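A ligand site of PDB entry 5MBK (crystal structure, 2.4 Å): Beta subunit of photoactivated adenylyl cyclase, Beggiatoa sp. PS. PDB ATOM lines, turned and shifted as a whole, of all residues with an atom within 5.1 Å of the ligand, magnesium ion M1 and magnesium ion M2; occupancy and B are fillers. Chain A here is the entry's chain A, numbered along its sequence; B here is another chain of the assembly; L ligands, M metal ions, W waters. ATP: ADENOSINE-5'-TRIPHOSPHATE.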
ATOM      1  N   ASP A 160       5.759  25.221   5.397  1.00  0.00           N
ATOM      2  CA  ASP A 160       4.513  24.588   5.796  1.00  0.00           C
ATOM      3  C   ASP A 160       3.367  25.520   5.452  1.00  0.00           C
ATOM      4  O   ASP A 160       3.461  26.725   5.715  1.00  0.00           O
ATOM      5  CB  ASP A 160       4.582  24.345   7.314  1.00  0.00           C
ATOM      6  CG  ASP A 160       3.438  23.569   7.821  1.00  0.00           C
ATOM      7  OD1 ASP A 160       2.335  24.101   7.829  1.00  0.00           O
ATOM      8  OD2 ASP A 160       3.685  22.421   8.259  1.00  0.00           O
ATOM      9  N   ILE A 161       2.266  24.965   4.915  1.00  0.00           N
ATOM     10  CA  ILE A 161       1.176  25.796   4.407  1.00  0.00           C
ATOM     11  C   ILE A 161       0.256  26.221   5.561  1.00  0.00           C
ATOM     12  O   ILE A 161      -0.126  25.423   6.424  1.00  0.00           O
ATOM     13  CB  ILE A 161       0.390  25.051   3.310  1.00  0.00           C
ATOM     14  CG1 ILE A 161       1.307  24.764   2.069  1.00  0.00           C
ATOM     15  CG2 ILE A 161      -0.872  25.844   2.976  1.00  0.00           C
ATOM     16  CD1 ILE A 161       0.659  23.743   1.015  1.00  0.00           C
ATOM     17  N   LEU A 162      -0.100  27.507   5.567  1.00  0.00           N
ATOM     18  CA  LEU A 162      -0.978  28.062   6.597  1.00  0.00           C
ATOM     19  C   LEU A 162      -2.375  27.508   6.407  1.00  0.00           C
ATOM     20  O   LEU A 162      -2.943  27.613   5.307  1.00  0.00           O
ATOM     21  CB  LEU A 162      -0.991  29.585   6.493  1.00  0.00           C
ATOM     22  CG  LEU A 162      -1.960  30.340   7.398  1.00  0.00           C
ATOM     23  CD1 LEU A 162      -1.423  30.286   8.816  1.00  0.00           C
ATOM     24  CD2 LEU A 162      -2.101  31.791   6.895  1.00  0.00           C
ATOM     25  N   ALA A 163      -2.910  26.879   7.462  1.00  0.00           N
ATOM     26  CA  ALA A 163      -4.317  26.438   7.498  1.00  0.00           C
ATOM     27  C   ALA A 163      -4.640  25.553   6.301  1.00  0.00           C
ATOM     28  O   ALA A 163      -5.682  25.699   5.659  1.00  0.00           O
ATOM     29  CB  ALA A 163      -5.273  27.647   7.555  1.00  0.00           C
ATOM     30  N   PHE A 164      -3.741  24.620   5.975  1.00  0.00           N
ATOM     31  CA  PHE A 164      -4.002  23.707   4.859  1.00  0.00           C
ATOM     32  C   PHE A 164      -5.292  22.906   5.043  1.00  0.00           C
ATOM     33  O   PHE A 164      -6.034  22.686   4.067  1.00  0.00           O
ATOM     34  CB  PHE A 164      -2.800  22.766   4.670  1.00  0.00           C
ATOM     35  CG  PHE A 164      -2.940  21.837   3.491  1.00  0.00           C
ATOM     36  CD1 PHE A 164      -2.500  22.222   2.232  1.00  0.00           C
ATOM     37  CD2 PHE A 164      -3.499  20.576   3.661  1.00  0.00           C
ATOM     38  CE1 PHE A 164      -2.625  21.385   1.165  1.00  0.00           C
ATOM     39  CE2 PHE A 164      -3.644  19.730   2.592  1.00  0.00           C
ATOM     40  CZ  PHE A 164      -3.204  20.132   1.347  1.00  0.00           C
ATOM     41  N   SER A 165      -5.612  22.456   6.269  1.00  0.00           N
ATOM     42  CA  SER A 165      -6.862  21.707   6.488  1.00  0.00           C
ATOM     43  C   SER A 165      -8.063  22.504   6.040  1.00  0.00           C
ATOM     44  O   SER A 165      -8.922  22.025   5.299  1.00  0.00           O
ATOM     45  CB  SER A 165      -7.030  21.358   7.956  1.00  0.00           C
ATOM     46  OG  SER A 165      -5.822  20.906   8.483  1.00  0.00           O
ATOM     47  N   THR A 166      -8.162  23.729   6.533  1.00  0.00           N
ATOM     48  CA  THR A 166      -9.238  24.638   6.195  1.00  0.00           C
ATOM     49  C   THR A 166      -9.237  24.975   4.712  1.00  0.00           C
ATOM     50  O   THR A 166     -10.297  25.013   4.066  1.00  0.00           O
ATOM     51  CB  THR A 166      -9.072  25.904   7.029  1.00  0.00           C
ATOM     52  OG1 THR A 166      -9.011  25.559   8.419  1.00  0.00           O
ATOM     53  CG2 THR A 166     -10.173  26.852   6.769  1.00  0.00           C
ATOM     54  N   ILE A 202       6.470  16.289   4.039  1.00  0.00           N
ATOM     55  CA  ILE A 202       5.676  15.805   5.144  1.00  0.00           C
ATOM     56  C   ILE A 202       4.340  16.544   5.086  1.00  0.00           C
ATOM     57  O   ILE A 202       4.211  17.631   5.651  1.00  0.00           O
ATOM     58  CB  ILE A 202       6.355  16.009   6.502  1.00  0.00           C
ATOM     59  CG1 ILE A 202       7.858  15.760   6.393  1.00  0.00           C
ATOM     60  CG2 ILE A 202       5.729  15.088   7.547  1.00  0.00           C
ATOM     61  CD1 ILE A 202       8.626  15.961   7.667  1.00  0.00           C
ATOM     62  N   GLY A 203       3.342  15.960   4.411  1.00  0.00           N
ATOM     63  CA  GLY A 203       2.031  16.567   4.370  1.00  0.00           C
ATOM     64  C   GLY A 203       2.029  17.795   3.489  1.00  0.00           C
ATOM     65  O   GLY A 203       2.252  17.727   2.276  1.00  0.00           O
ATOM     66  N   ASP A 204       1.777  18.952   4.095  1.00  0.00           N
ATOM     67  CA  ASP A 204       1.812  20.226   3.402  1.00  0.00           C
ATOM     68  C   ASP A 204       3.157  20.940   3.596  1.00  0.00           C
ATOM     69  O   ASP A 204       3.204  22.177   3.595  1.00  0.00           O
ATOM     70  CB  ASP A 204       0.674  21.114   3.902  1.00  0.00           C
ATOM     71  CG  ASP A 204       0.773  21.387   5.429  1.00  0.00           C
ATOM     72  OD1 ASP A 204       1.253  20.469   6.164  1.00  0.00           O
ATOM     73  OD2 ASP A 204       0.364  22.509   5.888  1.00  0.00           O
ATOM     74  N   CYS A 205       4.235  20.167   3.789  1.00  0.00           N
ATOM     75  CA  CYS A 205       5.458  20.665   4.400  1.00  0.00           C
ATOM     76  C   CYS A 205       6.719  20.186   3.678  1.00  0.00           C
ATOM     77  O   CYS A 205       6.836  19.012   3.312  1.00  0.00           O
ATOM     78  CB  CYS A 205       5.515  20.257   5.878  1.00  0.00           C
ATOM     79  SG  CYS A 205       7.110  20.409   6.589  1.00  0.00           S
ATOM     80  N   ARG A 287       3.144  31.220  12.763  1.00  0.00           N
ATOM     81  CA  ARG A 287       1.683  31.320  12.818  1.00  0.00           C
ATOM     82  C   ARG A 287       1.211  32.423  13.776  1.00  0.00           C
ATOM     83  O   ARG A 287       0.237  33.120  13.488  1.00  0.00           O
ATOM     84  CB  ARG A 287       1.054  29.984  13.242  1.00  0.00           C
ATOM     85  CG  ARG A 287       0.327  29.225  12.154  1.00  0.00           C
ATOM     86  CD  ARG A 287       1.184  29.151  10.920  1.00  0.00           C
ATOM     87  NE  ARG A 287       0.996  27.932  10.149  1.00  0.00           N
ATOM     88  CZ  ARG A 287       1.893  27.515   9.267  1.00  0.00           C
ATOM     89  NH1 ARG A 287       2.988  28.234   9.075  1.00  0.00           N
ATOM     90  NH2 ARG A 287       1.721  26.408   8.572  1.00  0.00           N
ATOM     91  N   PHE B 158       0.922   5.612  13.793  1.00  0.00           N
ATOM     92  CA  PHE B 158       2.115   6.387  14.122  1.00  0.00           C
ATOM     93  C   PHE B 158       2.766   5.723  15.326  1.00  0.00           C
ATOM     94  O   PHE B 158       2.100   5.460  16.338  1.00  0.00           O
ATOM     95  CB  PHE B 158       1.763   7.848  14.460  1.00  0.00           C
ATOM     96  CG  PHE B 158       2.100   8.811  13.375  1.00  0.00           C
ATOM     97  CD1 PHE B 158       1.262   8.995  12.298  1.00  0.00           C
ATOM     98  CD2 PHE B 158       3.259   9.562  13.429  1.00  0.00           C
ATOM     99  CE1 PHE B 158       1.563   9.926  11.293  1.00  0.00           C
ATOM    100  CE2 PHE B 158       3.577  10.494  12.443  1.00  0.00           C
ATOM    101  CZ  PHE B 158       2.722  10.669  11.376  1.00  0.00           C
ATOM    102  N   ILE B 202       9.827   9.123   9.903  1.00  0.00           N
ATOM    103  CA  ILE B 202       9.990  10.518  10.267  1.00  0.00           C
ATOM    104  C   ILE B 202      10.779  10.539  11.572  1.00  0.00           C
ATOM    105  O   ILE B 202      10.194  10.464  12.653  1.00  0.00           O
ATOM    106  CB  ILE B 202       8.646  11.240  10.428  1.00  0.00           C
ATOM    107  CG1 ILE B 202       7.649  10.772   9.370  1.00  0.00           C
ATOM    108  CG2 ILE B 202       8.856  12.751  10.341  1.00  0.00           C
ATOM    109  CD1 ILE B 202       6.291  11.407   9.455  1.00  0.00           C
ATOM    110  N   MET B 207       5.394   5.713  10.214  1.00  0.00           N
ATOM    111  CA  MET B 207       4.051   6.008   9.788  1.00  0.00           C
ATOM    112  C   MET B 207       3.571   4.887   8.892  1.00  0.00           C
ATOM    113  O   MET B 207       4.294   4.427   8.012  1.00  0.00           O
ATOM    114  CB  MET B 207       3.961   7.354   9.071  1.00  0.00           C
ATOM    115  CG  MET B 207       2.579   7.602   8.445  1.00  0.00           C
ATOM    116  SD  MET B 207       2.356   9.280   7.779  1.00  0.00           S
ATOM    117  CE  MET B 207       3.147   9.184   6.204  1.00  0.00           C
ATOM    118  N   THR B 270       2.159   9.109  -1.150  1.00  0.00           N
ATOM    119  CA  THR B 270       1.891   9.236   0.283  1.00  0.00           C
ATOM    120  C   THR B 270       0.401   9.446   0.533  1.00  0.00           C
ATOM    121  O   THR B 270      -0.432   9.330  -0.358  1.00  0.00           O
ATOM    122  CB  THR B 270       2.710  10.402   0.859  1.00  0.00           C
ATOM    123  OG1 THR B 270       2.614  10.397   2.298  1.00  0.00           O
ATOM    124  CG2 THR B 270       2.153  11.707   0.366  1.00  0.00           C
ATOM    125  N   LEU B 271       0.084   9.766   1.788  1.00  0.00           N
ATOM    126  CA  LEU B 271      -1.274   9.897   2.270  1.00  0.00           C
ATOM    127  C   LEU B 271      -1.377  11.268   2.909  1.00  0.00           C
ATOM    128  O   LEU B 271      -0.472  11.669   3.618  1.00  0.00           O
ATOM    129  CB  LEU B 271      -1.654   8.776   3.270  1.00  0.00           C
ATOM    130  CG  LEU B 271      -1.425   7.312   2.893  1.00  0.00           C
ATOM    131  CD1 LEU B 271      -1.488   6.394   4.107  1.00  0.00           C
ATOM    132  CD2 LEU B 271      -2.520   6.928   1.929  1.00  0.00           C
ATOM    133  N   LEU B 272      -2.456  11.988   2.587  1.00  0.00           N
ATOM    134  CA  LEU B 272      -2.716  13.348   3.064  1.00  0.00           C
ATOM    135  C   LEU B 272      -4.140  13.401   3.603  1.00  0.00           C
ATOM    136  O   LEU B 272      -5.077  12.915   2.945  1.00  0.00           O
ATOM    137  CB  LEU B 272      -2.501  14.374   1.926  1.00  0.00           C
ATOM    138  CG  LEU B 272      -2.572  15.884   2.168  1.00  0.00           C
ATOM    139  CD1 LEU B 272      -1.462  16.361   3.107  1.00  0.00           C
ATOM    140  CD2 LEU B 272      -2.493  16.657   0.863  1.00  0.00           C
ATOM    141  N   GLY B 273      -4.305  13.951   4.783  1.00  0.00           N
ATOM    142  CA  GLY B 273      -5.621  14.120   5.372  1.00  0.00           C
ATOM    143  C   GLY B 273      -5.427  14.390   6.842  1.00  0.00           C
ATOM    144  O   GLY B 273      -4.339  14.191   7.373  1.00  0.00           O
ATOM    145  N   ASP B 274      -6.517  14.857   7.484  1.00  0.00           N
ATOM    146  CA  ASP B 274      -6.472  15.206   8.928  1.00  0.00           C
ATOM    147  C   ASP B 274      -6.284  13.987   9.834  1.00  0.00           C
ATOM    148  O   ASP B 274      -5.672  14.109  10.888  1.00  0.00           O
ATOM    149  CB  ASP B 274      -7.769  15.938   9.355  1.00  0.00           C
ATOM    150  CG  ASP B 274      -7.895  17.350   8.732  1.00  0.00           C
ATOM    151  OD1 ASP B 274      -6.852  18.005   8.457  1.00  0.00           O
ATOM    152  OD2 ASP B 274      -9.050  17.800   8.505  1.00  0.00           O
ATOM    153  N   ALA B 275      -6.865  12.826   9.495  1.00  0.00           N
ATOM    154  CA  ALA B 275      -6.527  11.595  10.224  1.00  0.00           C
ATOM    155  C   ALA B 275      -5.034  11.471  10.472  1.00  0.00           C
ATOM    156  O   ALA B 275      -4.628  10.938  11.527  1.00  0.00           O
ATOM    157  CB  ALA B 275      -7.003  10.351   9.493  1.00  0.00           C
ATOM    158  N   VAL B 276      -4.188  11.940   9.537  1.00  0.00           N
ATOM    159  CA  VAL B 276      -2.758  11.799   9.756  1.00  0.00           C
ATOM    160  C   VAL B 276      -2.365  12.548  11.018  1.00  0.00           C
ATOM    161  O   VAL B 276      -1.749  12.000  11.947  1.00  0.00           O
ATOM    162  CB  VAL B 276      -1.964  12.259   8.528  1.00  0.00           C
ATOM    163  CG1 VAL B 276      -0.454  12.149   8.788  1.00  0.00           C
ATOM    164  CG2 VAL B 276      -2.386  11.426   7.331  1.00  0.00           C
ATOM    165  N   ASN B 277      -2.777  13.803  11.094  1.00  0.00           N
ATOM    166  CA  ASN B 277      -2.450  14.616  12.225  1.00  0.00           C
ATOM    167  C   ASN B 277      -2.968  14.021  13.530  1.00  0.00           C
ATOM    168  O   ASN B 277      -2.295  14.108  14.556  1.00  0.00           O
ATOM    169  CB  ASN B 277      -3.040  15.984  12.028  1.00  0.00           C
ATOM    170  CG  ASN B 277      -2.525  16.925  13.025  1.00  0.00           C
ATOM    171  OD1 ASN B 277      -1.411  17.411  12.871  1.00  0.00           O
ATOM    172  ND2 ASN B 277      -3.292  17.158  14.088  1.00  0.00           N
ATOM    173  N   ARG B 281      -0.937  12.881  17.039  1.00  0.00           N
ATOM    174  CA  ARG B 281      -1.190  13.409  18.382  1.00  0.00           C
ATOM    175  C   ARG B 281      -1.606  12.335  19.375  1.00  0.00           C
ATOM    176  O   ARG B 281      -1.280  12.463  20.564  1.00  0.00           O
ATOM    177  CB  ARG B 281      -2.282  14.489  18.396  1.00  0.00           C
ATOM    178  CG  ARG B 281      -2.092  15.547  17.364  1.00  0.00           C
ATOM    179  CD  ARG B 281      -1.048  16.566  17.791  1.00  0.00           C
ATOM    180  NE  ARG B 281      -1.071  17.754  16.951  1.00  0.00           N
ATOM    181  CZ  ARG B 281      -0.609  17.784  15.693  1.00  0.00           C
ATOM    182  NH1 ARG B 281      -0.659  18.914  14.989  1.00  0.00           N
ATOM    183  NH2 ARG B 281      -0.083  16.694  15.115  1.00  0.00           N
HETATM  184  PG  ATP L   1      -1.216  25.229  10.313  1.00  0.00           P
HETATM  185  O1G ATP L   1      -0.899  24.992  11.785  1.00  0.00           O
HETATM  186  O2G ATP L   1      -1.486  26.665   9.889  1.00  0.00           O
HETATM  187  O3G ATP L   1      -0.209  24.563   9.407  1.00  0.00           O
HETATM  188  PB  ATP L   1      -2.770  23.261   8.947  1.00  0.00           P
HETATM  189  O1B ATP L   1      -1.890  23.553   7.773  1.00  0.00           O
HETATM  190  O2B ATP L   1      -4.215  23.057   8.608  1.00  0.00           O
HETATM  191  O3B ATP L   1      -2.605  24.420  10.070  1.00  0.00           O
HETATM  192  PA  ATP L   1      -0.935  21.081   9.582  1.00  0.00           P
HETATM  193  O1A ATP L   1      -0.475  20.587  10.936  1.00  0.00           O
HETATM  194  O2A ATP L   1       0.047  21.825   8.712  1.00  0.00           O
HETATM  195  O3A ATP L   1      -2.275  21.973   9.779  1.00  0.00           O
HETATM  196  O5' ATP L   1      -1.548  19.846   8.737  1.00  0.00           O
HETATM  197  C5' ATP L   1      -1.849  19.918   7.348  1.00  0.00           C
HETATM  198  C4' ATP L   1      -2.177  18.541   6.788  1.00  0.00           C
HETATM  199  O4' ATP L   1      -0.975  17.755   6.679  1.00  0.00           O
HETATM  200  C3' ATP L   1      -3.151  17.780   7.685  1.00  0.00           C
HETATM  201  O3' ATP L   1      -4.198  17.228   6.869  1.00  0.00           O
HETATM  202  C2' ATP L   1      -2.251  16.743   8.350  1.00  0.00           C
HETATM  203  O2' ATP L   1      -2.853  15.539   8.804  1.00  0.00           O
HETATM  204  C1' ATP L   1      -1.280  16.473   7.235  1.00  0.00           C
HETATM  205  N9  ATP L   1      -0.082  15.807   7.764  1.00  0.00           N
HETATM  206  C8  ATP L   1       0.584  16.088   8.893  1.00  0.00           C
HETATM  207  N7  ATP L   1       1.650  15.274   9.031  1.00  0.00           N
HETATM  208  C5  ATP L   1       1.669  14.464   7.948  1.00  0.00           C
HETATM  209  C6  ATP L   1       2.496  13.343   7.456  1.00  0.00           C
HETATM  210  N6  ATP L   1       3.573  12.929   8.178  1.00  0.00           N
HETATM  211  N1  ATP L   1       2.148  12.763   6.272  1.00  0.00           N
HETATM  212  C2  ATP L   1       1.074  13.160   5.550  1.00  0.00           C
HETATM  213  N3  ATP L   1       0.254  14.157   5.946  1.00  0.00           N
HETATM  214  C4  ATP L   1       0.511  14.820   7.113  1.00  0.00           C
HETATM  215 MG    MG M   1       0.228  23.737   7.727  1.00  0.00          MG
HETATM  216 MG    MG M   2       1.994  20.759   8.297  1.00  0.00          MG
HETATM  217  O   HOH W   1       2.665  21.173  10.098  1.00  0.00           O
HETATM  218  O   HOH W   2      -6.228  24.634   9.443  1.00  0.00           O
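O of Gly 273 of chain B is in hydrogen-bond range of O2' of the ligand (2.5 Å). N of Ser 165 sits at hydrogen-bond distance from O2B of the ligand, at 2.8 Å. O2B of the ligand sits at hydrogen-bond distance from OG of Ser 165, at 2.7 Å. N of Phe 164 lies within hydrogen-bond range of O2B of the ligand (3.1 Å). The guanidinium group (NE) of Arg 287 is in salt-bridge range of an oxygen (O2G) of the ligand (2.8 Å). O2G of the ligand sits at hydrogen-bond distance from N of Ala 163 (2.8 Å). The backbone NH of Asn 277 of chain B lies within hydrogen-bond range of an oxygen (O2') of the ligand (2.9 Å). The backbone NH (N) of Asp 274 of chain B sits at hydrogen-bond distance from an oxygen (O3') of the ligand. An oxygen (O3') of the ligand sits at hydrogen-bond distance from the side-chain carboxylate of Asp 274 of chain B.
The backbone carbonyl oxygen (O) of Asp 160 is in hydrogen-bond range of the guanidinium group (NH2) of Arg 287, 3.4 Å away. The backbone carbonyl oxygen (O) of Ile 161 lies close to the guanidinium group (NH2) of Arg 287 (3.0 Å). OG of Ser 165 lies within hydrogen-bond range of OD1 of Asp 274 of chain B, 3.1 Å away.
The backbone carbonyl oxygen of Leu 271 of chain B lies close to a nitrogen (N3) of the ligand. Residues that only touch the ligand: Ile 202 of chain A (3.1 Å), Val 276 of chain B (3.3 Å), Ile 202 of chain B (3.4 Å), Gly 203 (3.4 Å), Leu 162 (3.6 Å), Met 207 of chain B (3.7 Å) and Leu 272 of chain B (3.9 Å). Hydrophobic or aromatic side chains that line the ligand: Leu 162, Phe 164, Ile 202 of chain A, Ile 202 of chain B, Met 207 of chain B, Leu 272 of chain B and Val 276 of chain B.
Arg 287 touches magnesium ion M1. Four residues have an atom within 4 Å of magnesium ion M1: Asp 160, Ile 161, Asp 204 and Arg 287. Along chain A the residues within 4 Å of magnesium ion M1 span positions 160 to 287.
Two residues have an atom within 4 Å of magnesium ion M2: Asp 160 and Asp 204. The nearest printed residue that does not touch magnesium ion M2 is Cys 205 (4.3 Å).
Magnesium ion M1 is bound by O3G of the ligand (1.9 Å), O1B of the ligand (2.1 Å), OD1 of Asp 160 (2.1 Å), O2A of the ligand (2.2 Å), O of Ile 161 (2.2 Å) and OD2 of Asp 204 (2.2 Å). Magnesium ion M1 has six donor atoms within binding distance.
Magnesium ion M2 is bound by water W1 (2.0 Å). Magnesium ion M2 is bound by an oxygen (O2A) of the ligand, 2.3 Å away. Magnesium ion M2 is bound by OD1 of Asp 204 (2.3 Å). The side-chain carboxylate (OD2) of Asp 160 is bound to magnesium ion M2 (2.4 Å).
Water W2 lies within hydrogen-bond range of an oxygen (O2B) of the ligand (2.7 Å) and the side-chain hydroxyl (OG1) of Thr 166 (3.1 Å).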
